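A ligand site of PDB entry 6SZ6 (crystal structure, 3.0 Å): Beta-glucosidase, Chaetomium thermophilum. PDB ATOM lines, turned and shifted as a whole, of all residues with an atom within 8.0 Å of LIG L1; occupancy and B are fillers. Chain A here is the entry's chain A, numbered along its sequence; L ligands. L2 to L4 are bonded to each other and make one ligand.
O of His 261 is in hydrogen-bond range of O5 of LIG L1 (2.5 Å).
O2 of LIG L1 is in hydrogen-bond range of OE1 of Glu 190 (2.9 Å).
O of His 234 lies within hydrogen-bond range of O5 of LG3 L3, at 3.1 Å.
Of the 12 residues printed, 2 come within 4 Å of LIG L1.
N of His 261 is in hydrogen-bond range of NE2 of His 234 (3.0 Å).
The side-chain hydroxyl (OH) of Tyr 231 is in hydrogen-bond range of the side-chain carboxylate (OE2) of Glu 190.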
ATOM      1  N   VAL A 182     -16.631 -20.497  -4.418  1.00  0.00           N
ATOM      2  CA  VAL A 182     -16.976 -19.413  -5.310  1.00  0.00           C
ATOM      3  C   VAL A 182     -17.180 -19.956  -6.722  1.00  0.00           C
ATOM      4  O   VAL A 182     -16.803 -21.083  -7.033  1.00  0.00           O
ATOM      5  CB  VAL A 182     -15.936 -18.271  -5.255  1.00  0.00           C
ATOM      6  CG1 VAL A 182     -15.718 -17.839  -3.826  1.00  0.00           C
ATOM      7  CG2 VAL A 182     -14.634 -18.723  -5.888  1.00  0.00           C
ATOM      8  N   ASP A 189     -17.758 -13.011  -4.734  1.00  0.00           N
ATOM      9  CA  ASP A 189     -16.317 -12.810  -4.669  1.00  0.00           C
ATOM     10  C   ASP A 189     -15.645 -13.731  -3.673  1.00  0.00           C
ATOM     11  O   ASP A 189     -14.473 -14.104  -3.862  1.00  0.00           O
ATOM     12  CB  ASP A 189     -15.992 -11.362  -4.310  1.00  0.00           C
ATOM     13  CG  ASP A 189     -16.565 -10.366  -5.284  1.00  0.00           C
ATOM     14  OD1 ASP A 189     -16.714 -10.723  -6.474  1.00  0.00           O
ATOM     15  OD2 ASP A 189     -16.884  -9.221  -4.868  1.00  0.00           O
ATOM     16  N   GLU A 190     -16.341 -14.101  -2.599  1.00  0.00           N
ATOM     17  CA  GLU A 190     -15.801 -15.004  -1.603  1.00  0.00           C
ATOM     18  C   GLU A 190     -16.894 -15.968  -1.165  1.00  0.00           C
ATOM     19  O   GLU A 190     -18.072 -15.804  -1.506  1.00  0.00           O
ATOM     20  CB  GLU A 190     -15.225 -14.249  -0.405  1.00  0.00           C
ATOM     21  CG  GLU A 190     -14.238 -13.142  -0.787  1.00  0.00           C
ATOM     22  CD  GLU A 190     -12.857 -13.653  -1.245  1.00  0.00           C
ATOM     23  OE1 GLU A 190     -11.996 -12.800  -1.525  1.00  0.00           O
ATOM     24  OE2 GLU A 190     -12.646 -14.890  -1.312  1.00  0.00           O
ATOM     25  N   TYR A 231     -12.126 -17.258   6.306  1.00  0.00           N
ATOM     26  CA  TYR A 231     -12.259 -18.684   6.063  1.00  0.00           C
ATOM     27  C   TYR A 231     -11.836 -19.490   7.284  1.00  0.00           C
ATOM     28  O   TYR A 231     -10.929 -19.116   8.014  1.00  0.00           O
ATOM     29  CB  TYR A 231     -11.407 -19.082   4.854  1.00  0.00           C
ATOM     30  CG  TYR A 231     -11.923 -18.539   3.536  1.00  0.00           C
ATOM     31  CD1 TYR A 231     -11.583 -17.259   3.107  1.00  0.00           C
ATOM     32  CD2 TYR A 231     -12.755 -19.299   2.718  1.00  0.00           C
ATOM     33  CE1 TYR A 231     -12.041 -16.760   1.903  1.00  0.00           C
ATOM     34  CE2 TYR A 231     -13.223 -18.803   1.523  1.00  0.00           C
ATOM     35  CZ  TYR A 231     -12.873 -17.531   1.115  1.00  0.00           C
ATOM     36  OH  TYR A 231     -13.332 -17.032  -0.079  1.00  0.00           O
ATOM     37  N   HIS A 234      -8.341 -20.012   7.711  1.00  0.00           N
ATOM     38  CA  HIS A 234      -7.515 -18.849   8.051  1.00  0.00           C
ATOM     39  C   HIS A 234      -8.014 -18.163   9.320  1.00  0.00           C
ATOM     40  O   HIS A 234      -7.744 -16.975   9.515  1.00  0.00           O
ATOM     41  CB  HIS A 234      -7.490 -17.797   6.936  1.00  0.00           C
ATOM     42  CG  HIS A 234      -7.374 -18.316   5.521  1.00  0.00           C
ATOM     43  ND1 HIS A 234      -7.429 -17.471   4.432  1.00  0.00           N
ATOM     44  CD2 HIS A 234      -7.199 -19.573   5.019  1.00  0.00           C
ATOM     45  CE1 HIS A 234      -7.299 -18.178   3.324  1.00  0.00           C
ATOM     46  NE2 HIS A 234      -7.164 -19.454   3.650  1.00  0.00           N
ATOM     47  N   GLN A 260      -7.911 -23.837   1.384  1.00  0.00           N
ATOM     48  CA  GLN A 260      -6.835 -22.916   1.736  1.00  0.00           C
ATOM     49  C   GLN A 260      -6.617 -21.926   0.595  1.00  0.00           C
ATOM     50  O   GLN A 260      -6.455 -22.336  -0.561  1.00  0.00           O
ATOM     51  CB  GLN A 260      -5.541 -23.664   2.036  1.00  0.00           C
ATOM     52  CG  GLN A 260      -4.294 -22.819   1.856  1.00  0.00           C
ATOM     53  CD  GLN A 260      -3.002 -23.608   1.984  1.00  0.00           C
ATOM     54  OE1 GLN A 260      -2.414 -23.671   3.063  1.00  0.00           O
ATOM     55  NE2 GLN A 260      -2.551 -24.196   0.875  1.00  0.00           N
ATOM     56  N   HIS A 261      -6.618 -20.630   0.922  1.00  0.00           N
ATOM     57  CA  HIS A 261      -6.419 -19.594  -0.079  1.00  0.00           C
ATOM     58  C   HIS A 261      -5.239 -18.681   0.221  1.00  0.00           C
ATOM     59  O   HIS A 261      -4.969 -17.759  -0.558  1.00  0.00           O
ATOM     60  CB  HIS A 261      -7.709 -18.772  -0.235  1.00  0.00           C
ATOM     61  CG  HIS A 261      -8.945 -19.601  -0.335  1.00  0.00           C
ATOM     62  ND1 HIS A 261      -9.038 -20.703  -1.145  1.00  0.00           N
ATOM     63  CD2 HIS A 261     -10.140 -19.504   0.304  1.00  0.00           C
ATOM     64  CE1 HIS A 261     -10.231 -21.254  -1.021  1.00  0.00           C
ATOM     65  NE2 HIS A 261     -10.923 -20.546  -0.139  1.00  0.00           N
ATOM     66  N   THR A 262      -4.507 -18.896   1.317  1.00  0.00           N
ATOM     67  CA  THR A 262      -3.324 -18.119   1.612  1.00  0.00           C
ATOM     68  C   THR A 262      -2.287 -19.019   2.266  1.00  0.00           C
ATOM     69  O   THR A 262      -2.639 -20.030   2.884  1.00  0.00           O
ATOM     70  CB  THR A 262      -3.659 -16.899   2.492  1.00  0.00           C
ATOM     71  OG1 THR A 262      -2.576 -15.952   2.453  1.00  0.00           O
ATOM     72  CG2 THR A 262      -3.919 -17.336   3.910  1.00  0.00           C
ATOM     73  N   GLY A 263      -1.015 -18.662   2.112  1.00  0.00           N
ATOM     74  CA  GLY A 263       0.061 -19.527   2.550  1.00  0.00           C
ATOM     75  C   GLY A 263       0.489 -19.341   3.987  1.00  0.00           C
ATOM     76  O   GLY A 263       0.141 -20.152   4.853  1.00  0.00           O
ATOM     77  N   PHE A 287       0.387 -22.884  -1.961  1.00  0.00           N
ATOM     78  CA  PHE A 287       0.588 -21.885  -0.915  1.00  0.00           C
ATOM     79  C   PHE A 287       1.620 -22.336   0.097  1.00  0.00           C
ATOM     80  O   PHE A 287       2.235 -21.522   0.779  1.00  0.00           O
ATOM     81  CB  PHE A 287      -0.715 -21.582  -0.197  1.00  0.00           C
ATOM     82  CG  PHE A 287      -1.750 -20.943  -1.062  1.00  0.00           C
ATOM     83  CD1 PHE A 287      -1.583 -19.648  -1.514  1.00  0.00           C
ATOM     84  CD2 PHE A 287      -2.881 -21.639  -1.420  1.00  0.00           C
ATOM     85  CE1 PHE A 287      -2.532 -19.065  -2.303  1.00  0.00           C
ATOM     86  CE2 PHE A 287      -3.816 -21.062  -2.218  1.00  0.00           C
ATOM     87  CZ  PHE A 287      -3.641 -19.763  -2.659  1.00  0.00           C
ATOM     88  N   ASP A 699       5.729 -15.367  -5.975  1.00  0.00           N
ATOM     89  CA  ASP A 699       4.570 -14.643  -5.481  1.00  0.00           C
ATOM     90  C   ASP A 699       4.697 -13.183  -5.870  1.00  0.00           C
ATOM     91  O   ASP A 699       5.641 -12.519  -5.448  1.00  0.00           O
ATOM     92  CB  ASP A 699       4.463 -14.777  -3.969  1.00  0.00           C
ATOM     93  CG  ASP A 699       3.252 -14.050  -3.389  1.00  0.00           C
ATOM     94  OD1 ASP A 699       2.589 -13.266  -4.108  1.00  0.00           O
ATOM     95  OD2 ASP A 699       2.961 -14.275  -2.186  1.00  0.00           O
ATOM     96  N   TYR A 701       3.257 -10.776  -4.707  1.00  0.00           N
ATOM     97  CA  TYR A 701       3.088  -9.978  -3.508  1.00  0.00           C
ATOM     98  C   TYR A 701       4.248 -10.142  -2.525  1.00  0.00           C
ATOM     99  O   TYR A 701       4.103  -9.821  -1.331  1.00  0.00           O
ATOM    100  CB  TYR A 701       1.755 -10.328  -2.836  1.00  0.00           C
ATOM    101  CG  TYR A 701       0.534  -9.628  -3.402  1.00  0.00           C
ATOM    102  CD1 TYR A 701      -0.587 -10.341  -3.800  1.00  0.00           C
ATOM    103  CD2 TYR A 701       0.513  -8.240  -3.545  1.00  0.00           C
ATOM    104  CE1 TYR A 701      -1.688  -9.695  -4.329  1.00  0.00           C
ATOM    105  CE2 TYR A 701      -0.582  -7.582  -4.062  1.00  0.00           C
ATOM    106  CZ  TYR A 701      -1.697  -8.314  -4.451  1.00  0.00           C
ATOM    107  OH  TYR A 701      -2.792  -7.656  -4.968  1.00  0.00           O
HETATM  108  C1  LIG L   1      -6.493 -12.064  -2.295  1.00  0.00           C
HETATM  109  C2  LIG L   1      -7.982 -11.776  -2.256  1.00  0.00           C
HETATM  110  C3  LIG L   1      -8.775 -13.108  -2.448  1.00  0.00           C
HETATM  111  C4  LIG L   1      -7.854 -14.304  -2.778  1.00  0.00           C
HETATM  112  C5  LIG L   1      -6.685 -14.403  -1.782  1.00  0.00           C
HETATM  113  C6  LIG L   1      -5.505 -15.171  -2.336  1.00  0.00           C
HETATM  114  O1  LIG L   1      -8.366 -10.852  -3.288  1.00  0.00           O
HETATM  115  O2  LIG L   1      -9.795 -13.012  -3.442  1.00  0.00           O
HETATM  116  O3  LIG L   1      -8.596 -15.516  -2.711  1.00  0.00           O
HETATM  117  O4  LIG L   1      -6.195 -13.100  -1.414  1.00  0.00           O
HETATM  118  O5  LIG L   1      -4.583 -15.343  -1.273  1.00  0.00           O
HETATM  119  C1  LG2 L   2      -5.998 -14.131   3.705  1.00  0.00           C
HETATM  120  C2  LG2 L   2      -6.229 -14.091   2.182  1.00  0.00           C
HETATM  121  C3  LG2 L   2      -6.444 -12.640   1.744  1.00  0.00           C
HETATM  122  C4  LG2 L   2      -7.238 -11.925   2.779  1.00  0.00           C
HETATM  123  C5  LG2 L   2      -6.353 -11.709   3.984  1.00  0.00           C
HETATM  124  C6  LG2 L   2      -7.149 -11.419   5.214  1.00  0.00           C
HETATM  125  O1  LG2 L   2      -7.427 -14.810   1.837  1.00  0.00           O
HETATM  126  O2  LG2 L   2      -7.133 -12.525   0.538  1.00  0.00           O
HETATM  127  O3  LG2 L   2      -7.663 -10.681   2.277  1.00  0.00           O
HETATM  128  O4  LG2 L   2      -5.545 -12.916   4.227  1.00  0.00           O
HETATM  129  O5  LG2 L   2      -6.329 -10.674   6.111  1.00  0.00           O
HETATM  130  C1  LG3 L   3      -6.617 -10.761   7.460  1.00  0.00           C
HETATM  131  C2  LG3 L   3      -5.628  -9.959   8.272  1.00  0.00           C
HETATM  132  C3  LG3 L   3      -4.280 -10.707   8.335  1.00  0.00           C
HETATM  133  C4  LG3 L   3      -4.460 -12.186   8.789  1.00  0.00           C
HETATM  134  C5  LG3 L   3      -5.575 -12.852   7.942  1.00  0.00           C
HETATM  135  C6  LG3 L   3      -5.978 -14.237   8.401  1.00  0.00           C
HETATM  136  O1  LG3 L   3      -6.091  -9.810   9.625  1.00  0.00           O
HETATM  137  O2  LG3 L   3      -3.359 -10.022   9.157  1.00  0.00           O
HETATM  138  O3  LG3 L   3      -3.243 -12.924   8.641  1.00  0.00           O
HETATM  139  O4  LG3 L   3      -6.764 -12.040   7.984  1.00  0.00           O
HETATM  140  O5  LG3 L   3      -7.160 -14.578   7.660  1.00  0.00           O
HETATM  141  C1  LG4 L   4      -7.104  -8.919   9.875  1.00  0.00           C
HETATM  142  C2  LG4 L   4      -6.827  -8.330  11.254  1.00  0.00           C
HETATM  143  C3  LG4 L   4      -6.996  -9.409  12.306  1.00  0.00           C
HETATM  144  C4  LG4 L   4      -8.333 -10.155  12.180  1.00  0.00           C
HETATM  145  C5  LG4 L   4      -8.668 -10.542  10.704  1.00  0.00           C
HETATM  146  C6  LG4 L   4     -10.127 -10.906  10.511  1.00  0.00           C
HETATM  147  O1  LG4 L   4      -7.788  -7.338  11.603  1.00  0.00           O
HETATM  148  O2  LG4 L   4      -6.899  -8.870  13.628  1.00  0.00           O
HETATM  149  O3  LG4 L   4      -8.258 -11.319  12.968  1.00  0.00           O
HETATM  150  O4  LG4 L   4      -8.404  -9.442   9.811  1.00  0.00           O
HETATM  151  O5  LG4 L   4     -10.322 -11.299   9.146  1.00  0.00           O
